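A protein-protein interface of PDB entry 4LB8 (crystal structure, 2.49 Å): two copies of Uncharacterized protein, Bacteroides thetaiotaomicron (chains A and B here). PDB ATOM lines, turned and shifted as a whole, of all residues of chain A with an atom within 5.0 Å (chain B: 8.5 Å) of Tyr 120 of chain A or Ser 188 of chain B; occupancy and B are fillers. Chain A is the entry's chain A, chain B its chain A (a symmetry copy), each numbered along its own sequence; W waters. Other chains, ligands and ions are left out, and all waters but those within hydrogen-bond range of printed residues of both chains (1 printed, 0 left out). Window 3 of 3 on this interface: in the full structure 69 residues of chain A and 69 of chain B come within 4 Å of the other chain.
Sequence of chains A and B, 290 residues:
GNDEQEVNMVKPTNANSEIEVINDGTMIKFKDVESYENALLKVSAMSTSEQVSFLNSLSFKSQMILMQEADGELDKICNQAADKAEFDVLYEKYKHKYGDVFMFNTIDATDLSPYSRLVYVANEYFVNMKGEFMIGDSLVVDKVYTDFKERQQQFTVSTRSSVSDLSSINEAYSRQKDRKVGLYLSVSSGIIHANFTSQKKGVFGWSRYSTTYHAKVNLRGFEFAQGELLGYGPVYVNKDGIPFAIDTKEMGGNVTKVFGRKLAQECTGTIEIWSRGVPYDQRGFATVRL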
ATOM      1  N   LEU A 118      -3.029  19.158  19.278  1.00  0.00           N
ATOM      2  CA  LEU A 118      -3.020  19.403  20.721  1.00  0.00           C
ATOM      3  C   LEU A 118      -1.847  18.802  21.462  1.00  0.00           C
ATOM      4  O   LEU A 118      -1.540  17.619  21.320  1.00  0.00           O
ATOM      5  CB  LEU A 118      -4.305  18.841  21.374  1.00  0.00           C
ATOM      6  CG  LEU A 118      -5.635  19.495  21.036  1.00  0.00           C
ATOM      7  CD1 LEU A 118      -6.754  18.853  21.816  1.00  0.00           C
ATOM      8  CD2 LEU A 118      -5.616  20.982  21.305  1.00  0.00           C
ATOM      9  N   VAL A 119      -1.257  19.604  22.336  1.00  0.00           N
ATOM     10  CA  VAL A 119      -0.191  19.167  23.240  1.00  0.00           C
ATOM     11  C   VAL A 119      -0.897  18.436  24.400  1.00  0.00           C
ATOM     12  O   VAL A 119      -0.528  17.317  24.758  1.00  0.00           O
ATOM     13  CB  VAL A 119       0.669  20.374  23.724  1.00  0.00           C
ATOM     14  CG1 VAL A 119       1.758  19.931  24.687  1.00  0.00           C
ATOM     15  CG2 VAL A 119       1.247  21.142  22.557  1.00  0.00           C
ATOM     16  N   TYR A 120      -1.946  19.071  24.944  1.00  0.00           N
ATOM     17  CA  TYR A 120      -2.761  18.568  26.048  1.00  0.00           C
ATOM     18  C   TYR A 120      -3.935  17.842  25.415  1.00  0.00           C
ATOM     19  O   TYR A 120      -5.022  18.383  25.225  1.00  0.00           O
ATOM     20  CB  TYR A 120      -3.153  19.741  26.967  1.00  0.00           C
ATOM     21  CG  TYR A 120      -1.969  20.630  27.313  1.00  0.00           C
ATOM     22  CD1 TYR A 120      -0.764  20.083  27.751  1.00  0.00           C
ATOM     23  CD2 TYR A 120      -2.036  22.011  27.159  1.00  0.00           C
ATOM     24  CE1 TYR A 120       0.342  20.883  28.010  1.00  0.00           C
ATOM     25  CE2 TYR A 120      -0.938  22.826  27.442  1.00  0.00           C
ATOM     26  CZ  TYR A 120       0.241  22.256  27.887  1.00  0.00           C
ATOM     27  OH  TYR A 120       1.327  23.032  28.203  1.00  0.00           O
ATOM     28  N   VAL A 121      -3.645  16.598  25.040  1.00  0.00           N
ATOM     29  CA  VAL A 121      -4.428  15.649  24.254  1.00  0.00           C
ATOM     30  C   VAL A 121      -5.878  15.426  24.728  1.00  0.00           C
ATOM     31  O   VAL A 121      -6.781  15.347  23.880  1.00  0.00           O
ATOM     32  CB  VAL A 121      -3.686  14.288  24.074  1.00  0.00           C
ATOM     33  CG1 VAL A 121      -2.451  14.465  23.214  1.00  0.00           C
ATOM     34  CG2 VAL A 121      -3.333  13.612  25.405  1.00  0.00           C
ATOM     35  N   ALA A 122      -6.102  15.292  26.053  1.00  0.00           N
ATOM     36  CA  ALA A 122      -7.441  14.998  26.593  1.00  0.00           C
ATOM     37  C   ALA A 122      -8.412  16.166  26.360  1.00  0.00           C
ATOM     38  O   ALA A 122      -9.601  15.942  26.350  1.00  0.00           O
ATOM     39  CB  ALA A 122      -7.370  14.626  28.064  1.00  0.00           C
ATOM     40  N   ASN A 123      -7.908  17.363  26.036  1.00  0.00           N
ATOM     41  CA  ASN A 123      -8.755  18.522  25.732  1.00  0.00           C
ATOM     42  C   ASN A 123      -9.577  18.343  24.431  1.00  0.00           C
ATOM     43  O   ASN A 123     -10.505  19.122  24.202  1.00  0.00           O
ATOM     44  CB  ASN A 123      -7.927  19.790  25.655  1.00  0.00           C
ATOM     45  CG  ASN A 123      -7.627  20.354  27.007  1.00  0.00           C
ATOM     46  OD1 ASN A 123      -8.354  20.120  27.953  1.00  0.00           O
ATOM     47  ND2 ASN A 123      -6.575  21.145  27.138  1.00  0.00           N
ATOM     48  N   GLU A 124      -9.260  17.301  23.616  1.00  0.00           N
ATOM     49  CA  GLU A 124      -9.944  16.939  22.366  1.00  0.00           C
ATOM     50  C   GLU A 124     -11.464  16.759  22.589  1.00  0.00           C
ATOM     51  O   GLU A 124     -12.253  17.043  21.687  1.00  0.00           O
ATOM     52  CB  GLU A 124      -9.336  15.668  21.739  1.00  0.00           C
ATOM     53  CG  GLU A 124      -9.513  14.376  22.536  1.00  0.00           C
ATOM     54  CD  GLU A 124      -9.503  13.084  21.739  1.00  0.00           C
ATOM     55  OE1 GLU A 124      -9.502  13.147  20.488  1.00  0.00           O
ATOM     56  OE2 GLU A 124      -9.532  12.003  22.369  1.00  0.00           O
ATOM     57  N   ASP A 142      -6.403  26.418  22.715  1.00  0.00           N
ATOM     58  CA  ASP A 142      -5.515  25.412  23.267  1.00  0.00           C
ATOM     59  C   ASP A 142      -4.218  25.249  22.483  1.00  0.00           C
ATOM     60  O   ASP A 142      -4.182  25.390  21.244  1.00  0.00           O
ATOM     61  CB  ASP A 142      -6.228  24.061  23.472  1.00  0.00           C
ATOM     62  CG  ASP A 142      -5.767  23.309  24.714  1.00  0.00           C
ATOM     63  OD1 ASP A 142      -5.488  23.967  25.744  1.00  0.00           O
ATOM     64  OD2 ASP A 142      -5.670  22.073  24.654  1.00  0.00           O
ATOM     65  N   LYS A 143      -3.136  24.994  23.271  1.00  0.00           N
ATOM     66  CA  LYS A 143      -1.755  24.772  22.828  1.00  0.00           C
ATOM     67  C   LYS A 143      -1.703  23.677  21.778  1.00  0.00           C
ATOM     68  O   LYS A 143      -2.226  22.573  21.981  1.00  0.00           O
ATOM     69  CB  LYS A 143      -0.818  24.427  24.014  1.00  0.00           C
ATOM     70  CG  LYS A 143       0.667  24.541  23.658  1.00  0.00           C
ATOM     71  CD  LYS A 143       1.590  24.505  24.861  1.00  0.00           C
ATOM     72  CE  LYS A 143       3.002  24.847  24.428  1.00  0.00           C
ATOM     73  NZ  LYS A 143       3.956  24.887  25.572  1.00  0.00           N
ATOM     74  N   LEU B 185       3.086  11.528  27.164  1.00  0.00           N
ATOM     75  CA  LEU B 185       2.703  12.328  28.330  1.00  0.00           C
ATOM     76  C   LEU B 185       3.033  13.789  28.168  1.00  0.00           C
ATOM     77  O   LEU B 185       4.093  14.143  27.638  1.00  0.00           O
ATOM     78  CB  LEU B 185       3.370  11.819  29.622  1.00  0.00           C
ATOM     79  CG  LEU B 185       3.108  10.369  30.040  1.00  0.00           C
ATOM     80  CD1 LEU B 185       3.829  10.078  31.323  1.00  0.00           C
ATOM     81  CD2 LEU B 185       1.602  10.048  30.144  1.00  0.00           C
ATOM     82  N   SER B 186       2.129  14.643  28.664  1.00  0.00           N
ATOM     83  CA  SER B 186       2.257  16.103  28.675  1.00  0.00           C
ATOM     84  C   SER B 186       1.572  16.624  29.939  1.00  0.00           C
ATOM     85  O   SER B 186       0.878  15.852  30.597  1.00  0.00           O
ATOM     86  CB  SER B 186       1.700  16.740  27.399  1.00  0.00           C
ATOM     87  OG  SER B 186       0.310  16.543  27.190  1.00  0.00           O
ATOM     88  N   VAL B 187       1.823  17.879  30.333  1.00  0.00           N
ATOM     89  CA  VAL B 187       1.231  18.400  31.573  1.00  0.00           C
ATOM     90  C   VAL B 187       0.775  19.848  31.383  1.00  0.00           C
ATOM     91  O   VAL B 187       1.531  20.683  30.870  1.00  0.00           O
ATOM     92  CB  VAL B 187       2.177  18.221  32.815  1.00  0.00           C
ATOM     93  CG1 VAL B 187       3.486  19.014  32.675  1.00  0.00           C
ATOM     94  CG2 VAL B 187       1.461  18.521  34.132  1.00  0.00           C
ATOM     95  N   SER B 188      -0.457  20.130  31.824  1.00  0.00           N
ATOM     96  CA  SER B 188      -1.087  21.461  31.792  1.00  0.00           C
ATOM     97  C   SER B 188      -1.552  21.813  33.171  1.00  0.00           C
ATOM     98  O   SER B 188      -2.537  21.231  33.648  1.00  0.00           O
ATOM     99  CB  SER B 188      -2.274  21.462  30.827  1.00  0.00           C
ATOM    100  OG  SER B 188      -2.946  22.706  30.728  1.00  0.00           O
ATOM    101  N   SER B 189      -0.842  22.736  33.839  1.00  0.00           N
ATOM    102  CA  SER B 189      -1.199  23.232  35.181  1.00  0.00           C
ATOM    103  C   SER B 189      -1.313  22.135  36.251  1.00  0.00           C
ATOM    104  O   SER B 189      -2.150  22.234  37.146  1.00  0.00           O
ATOM    105  CB  SER B 189      -2.500  24.026  35.132  1.00  0.00           C
ATOM    106  OG  SER B 189      -2.317  25.218  34.390  1.00  0.00           O
ATOM    107  N   GLY B 190      -0.432  21.146  36.188  1.00  0.00           N
ATOM    108  CA  GLY B 190      -0.393  20.061  37.152  1.00  0.00           C
ATOM    109  C   GLY B 190      -1.152  18.852  36.679  1.00  0.00           C
ATOM    110  O   GLY B 190      -0.939  17.770  37.224  1.00  0.00           O
ATOM    111  N   ILE B 191      -2.048  19.022  35.661  1.00  0.00           N
ATOM    112  CA  ILE B 191      -2.866  17.941  35.061  1.00  0.00           C
ATOM    113  C   ILE B 191      -2.048  17.266  33.985  1.00  0.00           C
ATOM    114  O   ILE B 191      -1.658  17.915  33.013  1.00  0.00           O
ATOM    115  CB  ILE B 191      -4.234  18.452  34.496  1.00  0.00           C
ATOM    116  CG1 ILE B 191      -5.065  19.279  35.533  1.00  0.00           C
ATOM    117  CG2 ILE B 191      -5.050  17.324  33.801  1.00  0.00           C
ATOM    118  CD1 ILE B 191      -5.636  18.533  36.689  1.00  0.00           C
ATOM    119  N   ILE B 192      -1.796  15.966  34.164  1.00  0.00           N
ATOM    120  CA  ILE B 192      -1.030  15.132  33.241  1.00  0.00           C
ATOM    121  C   ILE B 192      -1.991  14.480  32.235  1.00  0.00           C
ATOM    122  O   ILE B 192      -2.942  13.805  32.632  1.00  0.00           O
ATOM    123  CB  ILE B 192      -0.145  14.088  34.011  1.00  0.00           C
ATOM    124  CG1 ILE B 192       0.829  14.827  34.994  1.00  0.00           C
ATOM    125  CG2 ILE B 192       0.659  13.225  33.014  1.00  0.00           C
ATOM    126  CD1 ILE B 192       1.475  14.022  36.038  1.00  0.00           C
ATOM    127  N   HIS B 193      -1.726  14.701  30.933  1.00  0.00           N
ATOM    128  CA  HIS B 193      -2.485  14.186  29.796  1.00  0.00           C
ATOM    129  C   HIS B 193      -1.752  12.996  29.204  1.00  0.00           C
ATOM    130  O   HIS B 193      -0.549  13.083  28.992  1.00  0.00           O
ATOM    131  CB  HIS B 193      -2.624  15.292  28.729  1.00  0.00           C
ATOM    132  CG  HIS B 193      -3.623  16.358  29.063  1.00  0.00           C
ATOM    133  ND1 HIS B 193      -3.416  17.248  30.096  1.00  0.00           N
ATOM    134  CD2 HIS B 193      -4.778  16.671  28.442  1.00  0.00           C
ATOM    135  CE1 HIS B 193      -4.479  18.030  30.103  1.00  0.00           C
ATOM    136  NE2 HIS B 193      -5.319  17.722  29.118  1.00  0.00           N
ATOM    137  N   ALA B 194      -2.446  11.890  28.938  1.00  0.00           N
ATOM    138  CA  ALA B 194      -1.828  10.719  28.324  1.00  0.00           C
ATOM    139  C   ALA B 194      -2.495  10.430  27.008  1.00  0.00           C
ATOM    140  O   ALA B 194      -3.714  10.595  26.881  1.00  0.00           O
ATOM    141  CB  ALA B 194      -1.945   9.503  29.239  1.00  0.00           C
ATOM    142  N   ASN B 195      -1.700  10.003  26.039  1.00  0.00           N
ATOM    143  CA  ASN B 195      -2.146   9.582  24.728  1.00  0.00           C
ATOM    144  C   ASN B 195      -1.612   8.152  24.492  1.00  0.00           C
ATOM    145  O   ASN B 195      -0.404   7.926  24.509  1.00  0.00           O
ATOM    146  CB  ASN B 195      -1.697  10.578  23.634  1.00  0.00           C
ATOM    147  CG  ASN B 195      -2.295  10.398  22.243  1.00  0.00           C
ATOM    148  OD1 ASN B 195      -1.787  10.950  21.267  1.00  0.00           O
ATOM    149  ND2 ASN B 195      -3.358   9.626  22.088  1.00  0.00           N
ATOM    150  N   THR B 256      -7.270   9.253  24.590  1.00  0.00           N
ATOM    151  CA  THR B 256      -6.738  10.379  25.368  1.00  0.00           C
ATOM    152  C   THR B 256      -7.295  10.296  26.780  1.00  0.00           C
ATOM    153  O   THR B 256      -8.476  10.012  26.983  1.00  0.00           O
ATOM    154  CB  THR B 256      -6.971  11.723  24.709  1.00  0.00           C
ATOM    155  OG1 THR B 256      -8.363  12.041  24.726  1.00  0.00           O
ATOM    156  CG2 THR B 256      -6.375  11.803  23.300  1.00  0.00           C
ATOM    157  N   LYS B 257      -6.422  10.475  27.760  1.00  0.00           N
ATOM    158  CA  LYS B 257      -6.790  10.356  29.167  1.00  0.00           C
ATOM    159  C   LYS B 257      -6.095  11.380  30.048  1.00  0.00           C
ATOM    160  O   LYS B 257      -4.965  11.761  29.791  1.00  0.00           O
ATOM    161  CB  LYS B 257      -6.377   8.945  29.688  1.00  0.00           C
ATOM    162  CG  LYS B 257      -7.210   7.760  29.218  1.00  0.00           C
ATOM    163  CD  LYS B 257      -8.339   7.426  30.198  1.00  0.00           C
ATOM    164  CE  LYS B 257      -9.029   6.139  29.825  1.00  0.00           C
ATOM    165  NZ  LYS B 257     -10.484   6.157  30.135  1.00  0.00           N
ATOM    166  N   GLY B 260      -3.048  11.664  35.469  1.00  0.00           N
ATOM    167  CA  GLY B 260      -2.937  11.963  36.879  1.00  0.00           C
ATOM    168  C   GLY B 260      -2.657  13.426  37.095  1.00  0.00           C
ATOM    169  O   GLY B 260      -2.919  14.249  36.217  1.00  0.00           O
ATOM    170  N   ARG B 261      -2.139  13.752  38.275  1.00  0.00           N
ATOM    171  CA  ARG B 261      -1.725  15.100  38.658  1.00  0.00           C
ATOM    172  C   ARG B 261      -0.375  15.069  39.326  1.00  0.00           C
ATOM    173  O   ARG B 261      -0.013  14.053  39.926  1.00  0.00           O
ATOM    174  CB  ARG B 261      -2.716  15.728  39.656  1.00  0.00           C
ATOM    175  CG  ARG B 261      -4.006  16.264  39.089  1.00  0.00           C
ATOM    176  CD  ARG B 261      -4.774  17.090  40.110  1.00  0.00           C
ATOM    177  NE  ARG B 261      -5.129  16.340  41.323  1.00  0.00           N
ATOM    178  CZ  ARG B 261      -6.005  16.760  42.235  1.00  0.00           C
ATOM    179  NH1 ARG B 261      -6.662  17.900  42.060  1.00  0.00           N
ATOM    180  NH2 ARG B 261      -6.255  16.026  43.312  1.00  0.00           N
ATOM    181  N   LYS B 262       0.320  16.210  39.318  1.00  0.00           N
ATOM    182  CA  LYS B 262       1.558  16.419  40.052  1.00  0.00           C
ATOM    183  C   LYS B 262       1.244  16.813  41.525  1.00  0.00           C
ATOM    184  O   LYS B 262       0.404  17.691  41.788  1.00  0.00           O
ATOM    185  CB  LYS B 262       2.392  17.515  39.386  1.00  0.00           C
ATOM    186  CG  LYS B 262       3.002  17.133  38.045  1.00  0.00           C
ATOM    187  CD  LYS B 262       3.711  18.324  37.418  1.00  0.00           C
ATOM    188  CE  LYS B 262       4.870  18.817  38.250  1.00  0.00           C
ATOM    189  NZ  LYS B 262       5.543  19.982  37.634  1.00  0.00           N
ATOM    190  N   LEU B 290       8.186  15.794  34.201  1.00  0.00           N
ATOM    191  CA  LEU B 290       7.021  16.690  34.097  1.00  0.00           C
ATOM    192  C   LEU B 290       6.941  17.687  35.283  1.00  0.00           C
ATOM    193  O   LEU B 290       7.616  17.468  36.311  1.00  0.00           O
ATOM    194  CB  LEU B 290       5.698  15.874  33.984  1.00  0.00           C
ATOM    195  CG  LEU B 290       5.526  14.955  32.721  1.00  0.00           C
ATOM    196  CD1 LEU B 290       4.415  13.989  32.917  1.00  0.00           C
ATOM    197  CD2 LEU B 290       5.289  15.769  31.433  1.00  0.00           C
ATOM    198  OXT LEU B 290       6.244  18.715  35.158  1.00  0.00           O
HETATM  199  O   HOH W   1     -10.139   9.297  22.721  1.00  0.00           O
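Of chain B, only Ser 186, Val 187, Ser 188 and His 193 come within 4 Å of Tyr 120 of chain A.
Ser 188 of chain B touches just one residue of chain A: Tyr 120.
Val 121 of chain A touches just these residues of chain B: His 193, Ala 194, Asn 195 and Thr 256.
Printed residues of chain A within 4 Å of His 193 of chain B: Tyr 120 (3.4 Å), Val 121 (3.6 Å) and Ala 122 (3.1 Å).
Of the printed residues of chain A, Val 187 of chain B touches Tyr 120.
Printed residues of chain A within 4 Å of Ala 194 of chain B: Val 121 (3.4 Å).
Printed residues of chain B within 4 Å of Glu 124 of chain A: Thr 256 (2.6 Å).
The nearest residue of chain B that does not touch Tyr 120 of chain A is Ile 191 of chain B (5.8 Å).
The nearest printed residue of chain A that does not touch Ser 188 of chain B is Asn 123 of chain A (5.3 Å).
No position is printed for both chains.
OE2 of Glu 124 of chain A is in hydrogen-bond range of OG1 of Thr 256 of chain B (2.6 Å).
The backbone carbonyl oxygen of Val 119 of chain A sits at hydrogen-bond distance from the side-chain hydroxyl of Ser 186 of chain B, 2.7 Å away.
The backbone carbonyl oxygen (O) of Ile 191 of chain B lies within hydrogen-bond range of a ring nitrogen (ND1) of His 193 of chain B (3.5 Å).
N of His 193 of chain B sits at hydrogen-bond distance from O of Ser 186 of chain B (2.9 Å).
The backbone NH (N) of Ala 194 of chain B lies within hydrogen-bond range of the backbone carbonyl oxygen (O) of Lys 257 of chain B (2.7 Å).
N of Val 119 of chain A sits at hydrogen-bond distance from O of Lys 143 of chain A, at 3.1 Å.
Water W1 lies within hydrogen-bond range of OE2 of Glu 124 of chain A (2.8 Å) and N of Thr 256 of chain B (3.4 Å).
Of the 9 printed residues of chain A, 5 touch a printed residue of chain B.
Printed residues of chain A that touch a printed residue of chain B: Val 119, Tyr 120, Val 121, Ala 122 and Glu 124.
Hydrophobic or aromatic side chains of chain A within 4 Å of the printed part of chain B: Tyr 120, Val 121 and Ala 122.
Hydrophobic or aromatic side chains of chain B that line the printed part of chain A: His 193.
Among the printed residues, no Asp or Glu carboxylate lies within 4 Å of a Lys or Arg side-chain nitrogen of the other chain.
CD1 of Tyr 120 of chain A touches OG of Ser 186 of chain B (3.7 Å).
Tyr 120 of chain A touches Val 187 of chain B.
CG of Tyr 120 of chain A touches CB of Ser 188 of chain B, at 3.6 Å.
C of Tyr 120 of chain A touches CD2 of His 193 of chain B, at 3.4 Å.
His 193 of chain B touches Val 121 of chain A (CD2 to N, 3.6 Å).
O of Ala 194 of chain B touches CG2 of Val 121 of chain A, at 3.4 Å.
CG2 of Val 121 of chain A touches CB of Asn 195 of chain B, 3.9 Å away.
Val 121 of chain A touches Thr 256 of chain B (O to CG2, 3.6 Å).
His 193 of chain B touches Ala 122 of chain A.
Thr 256 of chain B touches Ala 122 of chain A.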
